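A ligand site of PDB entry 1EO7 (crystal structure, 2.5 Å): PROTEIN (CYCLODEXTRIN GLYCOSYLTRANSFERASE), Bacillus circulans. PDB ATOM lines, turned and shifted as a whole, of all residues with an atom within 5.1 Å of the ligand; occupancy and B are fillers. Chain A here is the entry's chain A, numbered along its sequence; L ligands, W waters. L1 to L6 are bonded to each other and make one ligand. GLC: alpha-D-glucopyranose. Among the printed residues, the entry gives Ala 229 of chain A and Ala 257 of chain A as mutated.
The backbone carbonyl oxygen of Tyr 195 sits at hydrogen-bond distance from an oxygen (O2) of GLC L6. A ring nitrogen (NE2) of His 140 sits close to an oxygen (O6) of GLC L1 (3.1 Å). An oxygen (O3) of GLC L1 sits at hydrogen-bond distance from the side-chain carboxylate (OD1) of Asp 328 (2.8 Å). The side-chain carboxylate (OD2) of Asp 371 sits at hydrogen-bond distance from an oxygen (O2) of GLC L3 (2.8 Å). The guanidinium group (NH2) of Arg 375 lies within hydrogen-bond range of an oxygen (O2) of GLC L2, 3.1 Å away. An oxygen (O1) of GLC L1 is in hydrogen-bond range of the guanidinium group of Arg 227 (2.7 Å). ND2 of Asn 193 lies close to O2 of GLC L6, at 3.1 Å. OG of Ser 145 lies within hydrogen-bond range of O4 of GLC L6 (3.1 Å). A ring nitrogen (NE2) of His 327 lies within hydrogen-bond range of an oxygen (O2) of GLC L1 (2.7 Å). The indole nitrogen (NE1) of Trp 101 sits at hydrogen-bond distance from an oxygen (O6) of GLC L2 (2.8 Å).
NH1 of Arg 227 lies within salt-bridge range of OD1 of Asp 135 (2.7 Å). The side-chain hydroxyl (OH) of Tyr 100 is in hydrogen-bond range of a ring nitrogen (NE2) of His 327, 3.3 Å away. The side-chain carboxylate (OD1) of Asp 371 lies within hydrogen-bond range of the side-chain hydroxyl (OH) of Tyr 97. The side-chain hydroxyl (OH) of Tyr 100 is in hydrogen-bond range of the side-chain carboxylate (OD2) of Asp 135, 2.9 Å away. N of Asn 193 sits at hydrogen-bond distance from O of Gly 179 (2.7 Å). The side-chain amide nitrogen (ND2) of Asn 193 lies within hydrogen-bond range of the side-chain hydroxyl (OH) of Tyr 167, 2.7 Å away. A ring nitrogen (NE2) of His 327 lies close to the side-chain carboxylate of Asp 328 (3.0 Å). The backbone carbonyl oxygen (O) of Asn 193 sits at hydrogen-bond distance from the backbone NH (N) of Thr 181 (3.3 Å).
Tyr 89 touches the ligand. His 98 touches the ligand. CD2 of Tyr 100 touches O2 of GLC L2 (3.3 Å). Ala 144 touches the ligand. Tyr 167 touches the ligand. Gly 179 touches the ligand. CA of Gly 180 touches O2 of GLC L6, at 3.6 Å. CD1 of Leu 194 touches C6 of GLC L1, at 3.5 Å. CA of Asp 196 touches O2 of GLC L6, 3.5 Å away. Leu 197 touches the ligand. Ala 229 touches the ligand. Ala 230 touches the ligand. Hydrophobic or aromatic side chains within 4 Å of the ligand: Tyr 89, His 98, Tyr 100, Trp 101, His 140, Tyr 167, Leu 194, Tyr 195, Leu 197, Ala 229 and His 327. Of the 29 residues printed, 22 come within 4 Å of the ligand. The nearest printed residue that does not touch the ligand is Thr 181 (4.4 Å).
Water W3 lies within hydrogen-bond range of an oxygen (O6) of GLC L3, the side-chain carboxylate of Asp 196 and the side-chain hydroxyl of Tyr 89. Water W2 lies within hydrogen-bond range of the backbone NH of Tyr 195 (2.7 Å), an oxygen (O3) of GLC L5 (2.9 Å), the backbone carbonyl oxygen of Thr 181 (3.0 Å) and the backbone carbonyl oxygen of Asn 193 (3.1 Å).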
ATOM      1  N   PHE A  21       1.093   8.882   1.417  1.00  0.00           N
ATOM      2  CA  PHE A  21      -0.055   9.560   0.861  1.00  0.00           C
ATOM      3  C   PHE A  21      -0.058   9.213  -0.605  1.00  0.00           C
ATOM      4  O   PHE A  21       0.513   9.936  -1.421  1.00  0.00           O
ATOM      5  CB  PHE A  21       0.067  11.069   1.041  1.00  0.00           C
ATOM      6  CG  PHE A  21      -1.219  11.748   1.455  1.00  0.00           C
ATOM      7  CD1 PHE A  21      -1.658  11.667   2.773  1.00  0.00           C
ATOM      8  CD2 PHE A  21      -1.983  12.440   0.536  1.00  0.00           C
ATOM      9  CE1 PHE A  21      -2.849  12.275   3.163  1.00  0.00           C
ATOM     10  CE2 PHE A  21      -3.171  13.057   0.926  1.00  0.00           C
ATOM     11  CZ  PHE A  21      -3.598  12.973   2.235  1.00  0.00           C
ATOM     12  N   TYR A  89     -15.408  24.086  -3.656  1.00  0.00           N
ATOM     13  CA  TYR A  89     -15.555  24.844  -2.430  1.00  0.00           C
ATOM     14  C   TYR A  89     -15.172  26.300  -2.633  1.00  0.00           C
ATOM     15  O   TYR A  89     -14.010  26.679  -2.458  1.00  0.00           O
ATOM     16  CB  TYR A  89     -14.727  24.222  -1.319  1.00  0.00           C
ATOM     17  CG  TYR A  89     -15.321  22.950  -0.766  1.00  0.00           C
ATOM     18  CD1 TYR A  89     -16.615  22.944  -0.256  1.00  0.00           C
ATOM     19  CD2 TYR A  89     -14.612  21.761  -0.783  1.00  0.00           C
ATOM     20  CE1 TYR A  89     -17.178  21.772   0.230  1.00  0.00           C
ATOM     21  CE2 TYR A  89     -15.156  20.603  -0.305  1.00  0.00           C
ATOM     22  CZ  TYR A  89     -16.424  20.608   0.209  1.00  0.00           C
ATOM     23  OH  TYR A  89     -16.944  19.429   0.682  1.00  0.00           O
ATOM     24  N   ASN A  94     -12.059  20.537  -5.598  1.00  0.00           N
ATOM     25  CA  ASN A  94     -11.505  19.552  -4.689  1.00  0.00           C
ATOM     26  C   ASN A  94     -11.815  18.137  -5.154  1.00  0.00           C
ATOM     27  O   ASN A  94     -12.926  17.851  -5.604  1.00  0.00           O
ATOM     28  CB  ASN A  94     -12.066  19.765  -3.273  1.00  0.00           C
ATOM     29  CG  ASN A  94     -11.450  20.955  -2.575  1.00  0.00           C
ATOM     30  OD1 ASN A  94     -10.490  20.819  -1.821  1.00  0.00           O
ATOM     31  ND2 ASN A  94     -12.012  22.131  -2.817  1.00  0.00           N
ATOM     32  N   TYR A  97      -8.682  12.889  -3.743  1.00  0.00           N
ATOM     33  CA  TYR A  97      -7.302  12.393  -3.860  1.00  0.00           C
ATOM     34  C   TYR A  97      -6.806  11.820  -2.539  1.00  0.00           C
ATOM     35  O   TYR A  97      -5.966  10.932  -2.517  1.00  0.00           O
ATOM     36  CB  TYR A  97      -6.382  13.524  -4.288  1.00  0.00           C
ATOM     37  CG  TYR A  97      -6.171  14.554  -3.208  1.00  0.00           C
ATOM     38  CD1 TYR A  97      -7.128  15.529  -2.966  1.00  0.00           C
ATOM     39  CD2 TYR A  97      -5.047  14.521  -2.388  1.00  0.00           C
ATOM     40  CE1 TYR A  97      -6.958  16.461  -1.953  1.00  0.00           C
ATOM     41  CE2 TYR A  97      -4.866  15.449  -1.384  1.00  0.00           C
ATOM     42  CZ  TYR A  97      -5.834  16.418  -1.163  1.00  0.00           C
ATOM     43  OH  TYR A  97      -5.664  17.341  -0.171  1.00  0.00           O
ATOM     44  N   HIS A  98      -7.310  12.363  -1.430  1.00  0.00           N
ATOM     45  CA  HIS A  98      -6.893  11.919  -0.102  1.00  0.00           C
ATOM     46  C   HIS A  98      -7.539  10.601   0.321  1.00  0.00           C
ATOM     47  O   HIS A  98      -7.130   9.975   1.294  1.00  0.00           O
ATOM     48  CB  HIS A  98      -7.154  13.016   0.951  1.00  0.00           C
ATOM     49  CG  HIS A  98      -8.496  13.662   0.820  1.00  0.00           C
ATOM     50  ND1 HIS A  98      -9.671  12.935   0.767  1.00  0.00           N
ATOM     51  CD2 HIS A  98      -8.855  14.963   0.730  1.00  0.00           C
ATOM     52  CE1 HIS A  98     -10.695  13.765   0.645  1.00  0.00           C
ATOM     53  NE2 HIS A  98     -10.225  15.002   0.620  1.00  0.00           N
ATOM     54  N   TYR A 100     -10.352  10.042   1.704  1.00  0.00           N
ATOM     55  CA  TYR A 100     -11.178  10.095   2.917  1.00  0.00           C
ATOM     56  C   TYR A 100     -12.678  10.230   2.643  1.00  0.00           C
ATOM     57  O   TYR A 100     -13.488  10.206   3.566  1.00  0.00           O
ATOM     58  CB  TYR A 100     -10.693  11.182   3.878  1.00  0.00           C
ATOM     59  CG  TYR A 100      -9.429  10.802   4.633  1.00  0.00           C
ATOM     60  CD1 TYR A 100      -9.402   9.681   5.467  1.00  0.00           C
ATOM     61  CD2 TYR A 100      -8.260  11.543   4.491  1.00  0.00           C
ATOM     62  CE1 TYR A 100      -8.247   9.329   6.143  1.00  0.00           C
ATOM     63  CE2 TYR A 100      -7.096  11.186   5.169  1.00  0.00           C
ATOM     64  CZ  TYR A 100      -7.107  10.072   5.987  1.00  0.00           C
ATOM     65  OH  TYR A 100      -5.993   9.713   6.697  1.00  0.00           O
ATOM     66  N   TRP A 101     -13.049  10.359   1.366  1.00  0.00           N
ATOM     67  CA  TRP A 101     -14.450  10.481   0.987  1.00  0.00           C
ATOM     68  C   TRP A 101     -14.968   9.192   0.377  1.00  0.00           C
ATOM     69  O   TRP A 101     -15.247   9.128  -0.823  1.00  0.00           O
ATOM     70  CB  TRP A 101     -14.649  11.637   0.023  1.00  0.00           C
ATOM     71  CG  TRP A 101     -14.221  12.910   0.609  1.00  0.00           C
ATOM     72  CD1 TRP A 101     -13.993  13.162   1.930  1.00  0.00           C
ATOM     73  CD2 TRP A 101     -13.933  14.131  -0.084  1.00  0.00           C
ATOM     74  NE1 TRP A 101     -13.585  14.457   2.097  1.00  0.00           N
ATOM     75  CE2 TRP A 101     -13.551  15.077   0.882  1.00  0.00           C
ATOM     76  CE3 TRP A 101     -13.978  14.510  -1.432  1.00  0.00           C
ATOM     77  CZ2 TRP A 101     -13.199  16.381   0.543  1.00  0.00           C
ATOM     78  CZ3 TRP A 101     -13.631  15.805  -1.761  1.00  0.00           C
ATOM     79  CH2 TRP A 101     -13.252  16.729  -0.775  1.00  0.00           C
ATOM     80  N   ASP A 135      -5.622   2.967   5.931  1.00  0.00           N
ATOM     81  CA  ASP A 135      -6.458   3.932   6.608  1.00  0.00           C
ATOM     82  C   ASP A 135      -7.900   3.469   6.520  1.00  0.00           C
ATOM     83  O   ASP A 135      -8.290   2.774   5.582  1.00  0.00           O
ATOM     84  CB  ASP A 135      -6.320   5.310   5.961  1.00  0.00           C
ATOM     85  CG  ASP A 135      -6.167   6.411   6.979  1.00  0.00           C
ATOM     86  OD1 ASP A 135      -7.150   6.622   7.690  1.00  0.00           O
ATOM     87  OD2 ASP A 135      -5.079   7.020   7.059  1.00  0.00           O
ATOM     88  N   ALA A 137     -11.797   5.127   7.426  1.00  0.00           N
ATOM     89  CA  ALA A 137     -12.660   6.190   7.916  1.00  0.00           C
ATOM     90  C   ALA A 137     -14.133   5.779   7.884  1.00  0.00           C
ATOM     91  O   ALA A 137     -14.895   6.250   7.048  1.00  0.00           O
ATOM     92  CB  ALA A 137     -12.452   7.461   7.109  1.00  0.00           C
ATOM     93  N   HIS A 140     -17.742   8.316   8.222  1.00  0.00           N
ATOM     94  CA  HIS A 140     -18.532   9.023   7.237  1.00  0.00           C
ATOM     95  C   HIS A 140     -18.237   8.506   5.861  1.00  0.00           C
ATOM     96  O   HIS A 140     -17.444   7.584   5.682  1.00  0.00           O
ATOM     97  CB  HIS A 140     -18.144  10.476   7.258  1.00  0.00           C
ATOM     98  CG  HIS A 140     -16.678  10.684   7.088  1.00  0.00           C
ATOM     99  ND1 HIS A 140     -15.813  10.808   8.148  1.00  0.00           N
ATOM    100  CD2 HIS A 140     -15.902  10.657   5.978  1.00  0.00           C
ATOM    101  CE1 HIS A 140     -14.575  10.920   7.710  1.00  0.00           C
ATOM    102  NE2 HIS A 140     -14.601  10.834   6.389  1.00  0.00           N
ATOM    103  N   ALA A 144     -21.699  16.263   1.803  1.00  0.00           N
ATOM    104  CA  ALA A 144     -23.041  16.229   1.272  1.00  0.00           C
ATOM    105  C   ALA A 144     -23.996  17.164   1.991  1.00  0.00           C
ATOM    106  O   ALA A 144     -23.794  17.523   3.145  1.00  0.00           O
ATOM    107  CB  ALA A 144     -23.581  14.816   1.267  1.00  0.00           C
ATOM    108  N   SER A 145     -25.059  17.544   1.289  1.00  0.00           N
ATOM    109  CA  SER A 145     -26.067  18.415   1.838  1.00  0.00           C
ATOM    110  C   SER A 145     -27.436  17.756   1.805  1.00  0.00           C
ATOM    111  O   SER A 145     -27.748  16.995   0.889  1.00  0.00           O
ATOM    112  CB  SER A 145     -26.111  19.733   1.081  1.00  0.00           C
ATOM    113  OG  SER A 145     -26.079  20.837   1.969  1.00  0.00           O
ATOM    114  N   TYR A 167     -27.683  10.896   1.963  1.00  0.00           N
ATOM    115  CA  TYR A 167     -27.990  11.837   3.030  1.00  0.00           C
ATOM    116  C   TYR A 167     -29.391  12.434   2.869  1.00  0.00           C
ATOM    117  O   TYR A 167     -30.115  12.610   3.845  1.00  0.00           O
ATOM    118  CB  TYR A 167     -26.954  12.958   3.067  1.00  0.00           C
ATOM    119  CG  TYR A 167     -26.778  13.596   4.427  1.00  0.00           C
ATOM    120  CD1 TYR A 167     -26.522  12.819   5.549  1.00  0.00           C
ATOM    121  CD2 TYR A 167     -26.860  14.975   4.585  1.00  0.00           C
ATOM    122  CE1 TYR A 167     -26.360  13.406   6.796  1.00  0.00           C
ATOM    123  CE2 TYR A 167     -26.697  15.561   5.822  1.00  0.00           C
ATOM    124  CZ  TYR A 167     -26.451  14.778   6.922  1.00  0.00           C
ATOM    125  OH  TYR A 167     -26.283  15.374   8.150  1.00  0.00           O
ATOM    126  N   GLY A 179     -26.790  18.232  11.924  1.00  0.00           N
ATOM    127  CA  GLY A 179     -25.915  19.277  11.419  1.00  0.00           C
ATOM    128  C   GLY A 179     -24.444  18.960  11.670  1.00  0.00           C
ATOM    129  O   GLY A 179     -24.061  17.806  11.863  1.00  0.00           O
ATOM    130  N   GLY A 180     -23.622  19.998  11.662  1.00  0.00           N
ATOM    131  CA  GLY A 180     -22.200  19.856  11.863  1.00  0.00           C
ATOM    132  C   GLY A 180     -21.781  20.163  13.296  1.00  0.00           C
ATOM    133  O   GLY A 180     -22.503  20.806  14.055  1.00  0.00           O
ATOM    134  N   THR A 181     -20.587  19.695  13.645  1.00  0.00           N
ATOM    135  CA  THR A 181     -20.022  19.884  14.961  1.00  0.00           C
ATOM    136  C   THR A 181     -19.136  21.110  14.982  1.00  0.00           C
ATOM    137  O   THR A 181     -18.651  21.567  13.943  1.00  0.00           O
ATOM    138  CB  THR A 181     -19.159  18.672  15.353  1.00  0.00           C
ATOM    139  OG1 THR A 181     -18.453  18.950  16.569  1.00  0.00           O
ATOM    140  CG2 THR A 181     -18.139  18.371  14.254  1.00  0.00           C
ATOM    141  N   ASN A 193     -21.954  16.061  12.066  1.00  0.00           N
ATOM    142  CA  ASN A 193     -21.135  15.892  10.862  1.00  0.00           C
ATOM    143  C   ASN A 193     -19.735  16.456  11.003  1.00  0.00           C
ATOM    144  O   ASN A 193     -19.555  17.657  11.245  1.00  0.00           O
ATOM    145  CB  ASN A 193     -21.814  16.545   9.663  1.00  0.00           C
ATOM    146  CG  ASN A 193     -22.958  15.726   9.120  1.00  0.00           C
ATOM    147  OD1 ASN A 193     -23.166  14.585   9.532  1.00  0.00           O
ATOM    148  ND2 ASN A 193     -23.715  16.307   8.203  1.00  0.00           N
ATOM    149  N   LEU A 194     -18.733  15.601  10.797  1.00  0.00           N
ATOM    150  CA  LEU A 194     -17.349  16.059  10.825  1.00  0.00           C
ATOM    151  C   LEU A 194     -17.213  17.014   9.644  1.00  0.00           C
ATOM    152  O   LEU A 194     -17.149  16.588   8.503  1.00  0.00           O
ATOM    153  CB  LEU A 194     -16.393  14.874  10.655  1.00  0.00           C
ATOM    154  CG  LEU A 194     -14.988  15.053  11.246  1.00  0.00           C
ATOM    155  CD1 LEU A 194     -13.954  14.398  10.355  1.00  0.00           C
ATOM    156  CD2 LEU A 194     -14.678  16.539  11.425  1.00  0.00           C
ATOM    157  N   TYR A 195     -17.232  18.305   9.924  1.00  0.00           N
ATOM    158  CA  TYR A 195     -17.242  19.292   8.851  1.00  0.00           C
ATOM    159  C   TYR A 195     -18.553  19.009   8.094  1.00  0.00           C
ATOM    160  O   TYR A 195     -19.596  18.807   8.707  1.00  0.00           O
ATOM    161  CB  TYR A 195     -16.037  19.110   7.933  1.00  0.00           C
ATOM    162  CG  TYR A 195     -14.740  19.648   8.493  1.00  0.00           C
ATOM    163  CD1 TYR A 195     -14.603  21.004   8.797  1.00  0.00           C
ATOM    164  CD2 TYR A 195     -13.654  18.820   8.716  1.00  0.00           C
ATOM    165  CE1 TYR A 195     -13.423  21.506   9.308  1.00  0.00           C
ATOM    166  CE2 TYR A 195     -12.464  19.319   9.228  1.00  0.00           C
ATOM    167  CZ  TYR A 195     -12.352  20.664   9.519  1.00  0.00           C
ATOM    168  OH  TYR A 195     -11.176  21.157  10.029  1.00  0.00           O
ATOM    169  N   ASP A 196     -18.481  18.926   6.779  1.00  0.00           N
ATOM    170  CA  ASP A 196     -19.651  18.598   5.985  1.00  0.00           C
ATOM    171  C   ASP A 196     -19.704  17.085   5.573  1.00  0.00           C
ATOM    172  O   ASP A 196     -20.470  16.715   4.683  1.00  0.00           O
ATOM    173  CB  ASP A 196     -19.706  19.440   4.743  1.00  0.00           C
ATOM    174  CG  ASP A 196     -18.613  19.102   3.778  1.00  0.00           C
ATOM    175  OD1 ASP A 196     -17.626  18.445   4.166  1.00  0.00           O
ATOM    176  OD2 ASP A 196     -18.785  19.457   2.603  1.00  0.00           O
ATOM    177  N   LEU A 197     -18.903  16.241   6.216  1.00  0.00           N
ATOM    178  CA  LEU A 197     -18.888  14.815   5.876  1.00  0.00           C
ATOM    179  C   LEU A 197     -20.118  14.087   6.422  1.00  0.00           C
ATOM    180  O   LEU A 197     -20.415  14.162   7.610  1.00  0.00           O
ATOM    181  CB  LEU A 197     -17.611  14.140   6.392  1.00  0.00           C
ATOM    182  CG  LEU A 197     -16.287  14.659   5.812  1.00  0.00           C
ATOM    183  CD1 LEU A 197     -15.120  13.833   6.342  1.00  0.00           C
ATOM    184  CD2 LEU A 197     -16.322  14.632   4.297  1.00  0.00           C
ATOM    185  N   ARG A 227      -5.374   1.906  10.498  1.00  0.00           N
ATOM    186  CA  ARG A 227      -5.313   3.234  11.054  1.00  0.00           C
ATOM    187  C   ARG A 227      -6.705   3.833  10.976  1.00  0.00           C
ATOM    188  O   ARG A 227      -7.193   4.151   9.891  1.00  0.00           O
ATOM    189  CB  ARG A 227      -4.323   4.116  10.295  1.00  0.00           C
ATOM    190  CG  ARG A 227      -4.163   5.510  10.887  1.00  0.00           C
ATOM    191  CD  ARG A 227      -5.220   6.473  10.374  1.00  0.00           C
ATOM    192  NE  ARG A 227      -4.824   7.871  10.538  1.00  0.00           N
ATOM    193  CZ  ARG A 227      -5.541   8.885  10.089  1.00  0.00           C
ATOM    194  NH1 ARG A 227      -6.632   8.614   9.429  1.00  0.00           N
ATOM    195  NH2 ARG A 227      -5.125  10.145  10.248  1.00  0.00           N
ATOM    196  N   ALA A 229      -9.347   6.563  11.205  1.00  0.00           N
ATOM    197  CA  ALA A 229      -9.518   7.993  11.094  1.00  0.00           C
ATOM    198  C   ALA A 229     -10.633   8.441  12.015  1.00  0.00           C
ATOM    199  O   ALA A 229     -11.534   7.656  12.341  1.00  0.00           O
ATOM    200  CB  ALA A 229      -9.872   8.341   9.677  1.00  0.00           C
ATOM    201  N   ALA A 230     -10.591   9.711  12.406  1.00  0.00           N
ATOM    202  CA  ALA A 230     -11.596  10.346  13.261  1.00  0.00           C
ATOM    203  C   ALA A 230     -12.162   9.463  14.372  1.00  0.00           C
ATOM    204  O   ALA A 230     -13.376   9.379  14.531  1.00  0.00           O
ATOM    205  CB  ALA A 230     -12.718  10.921  12.417  1.00  0.00           C
ATOM    206  N   ALA A 257      -6.764   7.903  15.127  1.00  0.00           N
ATOM    207  CA  ALA A 257      -6.269   9.253  15.034  1.00  0.00           C
ATOM    208  C   ALA A 257      -7.121  10.149  15.901  1.00  0.00           C
ATOM    209  O   ALA A 257      -8.237  10.488  15.546  1.00  0.00           O
ATOM    210  CB  ALA A 257      -6.289   9.735  13.598  1.00  0.00           C
ATOM    211  N   HIS A 327      -0.124  14.589   7.576  1.00  0.00           N
ATOM    212  CA  HIS A 327      -0.939  15.254   6.567  1.00  0.00           C
ATOM    213  C   HIS A 327      -1.893  16.304   7.174  1.00  0.00           C
ATOM    214  O   HIS A 327      -2.434  17.132   6.452  1.00  0.00           O
ATOM    215  CB  HIS A 327      -1.741  14.211   5.777  1.00  0.00           C
ATOM    216  CG  HIS A 327      -2.663  13.394   6.618  1.00  0.00           C
ATOM    217  ND1 HIS A 327      -2.219  12.423   7.498  1.00  0.00           N
ATOM    218  CD2 HIS A 327      -3.998  13.417   6.716  1.00  0.00           C
ATOM    219  CE1 HIS A 327      -3.257  11.884   8.094  1.00  0.00           C
ATOM    220  NE2 HIS A 327      -4.343  12.456   7.620  1.00  0.00           N
ATOM    221  N   ASP A 328      -2.106  16.238   8.498  1.00  0.00           N
ATOM    222  CA  ASP A 328      -3.018  17.193   9.143  1.00  0.00           C
ATOM    223  C   ASP A 328      -2.309  18.392   9.764  1.00  0.00           C
ATOM    224  O   ASP A 328      -2.941  19.209  10.425  1.00  0.00           O
ATOM    225  CB  ASP A 328      -3.847  16.517  10.250  1.00  0.00           C
ATOM    226  CG  ASP A 328      -4.430  15.200   9.822  1.00  0.00           C
ATOM    227  OD1 ASP A 328      -5.001  15.131   8.717  1.00  0.00           O
ATOM    228  OD2 ASP A 328      -4.416  14.248  10.633  1.00  0.00           O
ATOM    229  N   ASP A 371      -2.695  21.647   5.319  1.00  0.00           N
ATOM    230  CA  ASP A 371      -3.243  21.000   4.131  1.00  0.00           C
ATOM    231  C   ASP A 371      -3.901  22.018   3.196  1.00  0.00           C
ATOM    232  O   ASP A 371      -4.532  22.966   3.654  1.00  0.00           O
ATOM    233  CB  ASP A 371      -4.210  19.889   4.562  1.00  0.00           C
ATOM    234  CG  ASP A 371      -5.406  19.732   3.630  1.00  0.00           C
ATOM    235  OD1 ASP A 371      -5.235  19.635   2.412  1.00  0.00           O
ATOM    236  OD2 ASP A 371      -6.526  19.665   4.128  1.00  0.00           O
ATOM    237  N   ARG A 375       0.919  18.279   1.565  1.00  0.00           N
ATOM    238  CA  ARG A 375       0.752  17.060   0.798  1.00  0.00           C
ATOM    239  C   ARG A 375       1.366  17.138  -0.592  1.00  0.00           C
ATOM    240  O   ARG A 375       0.857  16.547  -1.541  1.00  0.00           O
ATOM    241  CB  ARG A 375      -0.717  16.663   0.706  1.00  0.00           C
ATOM    242  CG  ARG A 375      -1.336  16.288   2.037  1.00  0.00           C
ATOM    243  CD  ARG A 375      -2.704  16.906   2.196  1.00  0.00           C
ATOM    244  NE  ARG A 375      -3.260  16.656   3.526  1.00  0.00           N
ATOM    245  CZ  ARG A 375      -4.523  16.319   3.740  1.00  0.00           C
ATOM    246  NH1 ARG A 375      -5.362  16.171   2.724  1.00  0.00           N
ATOM    247  NH2 ARG A 375      -4.947  16.117   4.990  1.00  0.00           N
HETATM  248  C1  GLC L   1      -8.578  11.996   9.360  1.00  0.00           C
HETATM  249  C2  GLC L   1      -7.544  12.450   8.379  1.00  0.00           C
HETATM  250  C3  GLC L   1      -7.854  13.832   7.861  1.00  0.00           C
HETATM  251  C4  GLC L   1      -9.224  13.629   7.266  1.00  0.00           C
HETATM  252  C5  GLC L   1     -10.224  13.389   8.393  1.00  0.00           C
HETATM  253  C6  GLC L   1     -11.662  13.400   7.958  1.00  0.00           C
HETATM  254  O1  GLC L   1      -8.339  10.670   9.784  1.00  0.00           O
HETATM  255  O2  GLC L   1      -6.445  12.273   9.247  1.00  0.00           O
HETATM  256  O3  GLC L   1      -6.827  14.125   6.911  1.00  0.00           O
HETATM  257  O4  GLC L   1      -9.491  14.871   6.605  1.00  0.00           O
HETATM  258  O5  GLC L   1      -9.883  12.085   8.854  1.00  0.00           O
HETATM  259  O6  GLC L   1     -11.922  12.360   7.013  1.00  0.00           O
HETATM  260  C1  GLC L   2      -9.984  14.553   5.323  1.00  0.00           C
HETATM  261  C2  GLC L   2      -9.029  15.223   4.367  1.00  0.00           C
HETATM  262  C3  GLC L   2      -9.053  16.717   4.534  1.00  0.00           C
HETATM  263  C4  GLC L   2     -10.473  17.251   4.462  1.00  0.00           C
HETATM  264  C5  GLC L   2     -11.384  16.509   5.425  1.00  0.00           C
HETATM  265  C6  GLC L   2     -12.817  16.882   5.220  1.00  0.00           C
HETATM  266  O2  GLC L   2      -7.701  14.749   4.424  1.00  0.00           O
HETATM  267  O3  GLC L   2      -8.290  17.341   3.497  1.00  0.00           O
HETATM  268  O4  GLC L   2     -10.421  18.622   4.915  1.00  0.00           O
HETATM  269  O5  GLC L   2     -11.286  15.094   5.219  1.00  0.00           O
HETATM  270  O6  GLC L   2     -13.209  16.646   3.872  1.00  0.00           O
HETATM  271  C1  GLC L   3      -9.797  19.613   4.126  1.00  0.00           C
HETATM  272  C2  GLC L   3      -9.403  20.751   5.042  1.00  0.00           C
HETATM  273  C3  GLC L   3     -10.627  21.313   5.710  1.00  0.00           C
HETATM  274  C4  GLC L   3     -11.602  21.787   4.647  1.00  0.00           C
HETATM  275  C5  GLC L   3     -11.887  20.686   3.637  1.00  0.00           C
HETATM  276  C6  GLC L   3     -12.613  21.259   2.452  1.00  0.00           C
HETATM  277  O2  GLC L   3      -8.455  20.359   6.009  1.00  0.00           O
HETATM  278  O3  GLC L   3     -10.299  22.441   6.534  1.00  0.00           O
HETATM  279  O4  GLC L   3     -12.835  22.115   5.306  1.00  0.00           O
HETATM  280  O5  GLC L   3     -10.693  20.094   3.136  1.00  0.00           O
HETATM  281  O6  GLC L   3     -13.957  20.776   2.380  1.00  0.00           O
HETATM  282  C1  GLC L   4     -13.472  23.329   4.950  1.00  0.00           C
HETATM  283  C2  GLC L   4     -13.610  24.169   6.197  1.00  0.00           C
HETATM  284  C3  GLC L   4     -14.809  23.780   7.019  1.00  0.00           C
HETATM  285  C4  GLC L   4     -16.046  23.657   6.152  1.00  0.00           C
HETATM  286  C5  GLC L   4     -15.795  22.666   5.035  1.00  0.00           C
HETATM  287  C6  GLC L   4     -16.981  22.568   4.125  1.00  0.00           C
HETATM  288  O2  GLC L   4     -12.428  24.049   6.977  1.00  0.00           O
HETATM  289  O3  GLC L   4     -15.100  24.761   8.028  1.00  0.00           O
HETATM  290  O4  GLC L   4     -17.105  23.166   6.997  1.00  0.00           O
HETATM  291  O5  GLC L   4     -14.691  23.103   4.248  1.00  0.00           O
HETATM  292  O6  GLC L   4     -17.523  23.858   3.845  1.00  0.00           O
HETATM  293  C1  GLC L   5     -18.068  24.100   7.432  1.00  0.00           C
HETATM  294  C2  GLC L   5     -18.610  23.649   8.766  1.00  0.00           C
HETATM  295  C3  GLC L   5     -19.506  22.447   8.600  1.00  0.00           C
HETATM  296  C4  GLC L   5     -20.579  22.753   7.573  1.00  0.00           C
HETATM  297  C5  GLC L   5     -19.929  23.126   6.247  1.00  0.00           C
HETATM  298  C6  GLC L   5     -20.955  23.521   5.227  1.00  0.00           C
HETATM  299  O2  GLC L   5     -17.535  23.340   9.641  1.00  0.00           O
HETATM  300  O3  GLC L   5     -20.182  22.101   9.821  1.00  0.00           O
HETATM  301  O4  GLC L   5     -21.407  21.586   7.419  1.00  0.00           O
HETATM  302  O5  GLC L   5     -19.078  24.259   6.446  1.00  0.00           O
HETATM  303  O6  GLC L   5     -21.741  24.607   5.709  1.00  0.00           O
HETATM  304  C1  GLC L   6     -22.551  21.479   8.227  1.00  0.00           C
HETATM  305  C2  GLC L   6     -23.197  20.122   8.012  1.00  0.00           C
HETATM  306  C3  GLC L   6     -23.668  19.978   6.580  1.00  0.00           C
HETATM  307  C4  GLC L   6     -24.513  21.163   6.140  1.00  0.00           C
HETATM  308  C5  GLC L   6     -23.862  22.487   6.508  1.00  0.00           C
HETATM  309  C6  GLC L   6     -24.788  23.639   6.277  1.00  0.00           C
HETATM  310  O2  GLC L   6     -22.267  19.093   8.333  1.00  0.00           O
HETATM  311  O3  GLC L   6     -24.465  18.809   6.430  1.00  0.00           O
HETATM  312  O4  GLC L   6     -24.660  21.197   4.728  1.00  0.00           O
HETATM  313  O5  GLC L   6     -23.481  22.499   7.886  1.00  0.00           O
HETATM  314  O6  GLC L   6     -25.987  23.492   7.047  1.00  0.00           O
HETATM  315  O   HOH W   1      -8.113  18.167   7.591  1.00  0.00           O
HETATM  316  O   HOH W   2     -18.216  20.455  11.196  1.00  0.00           O
HETATM  317  O   HOH W   3     -15.072  18.451   3.140  1.00  0.00           O
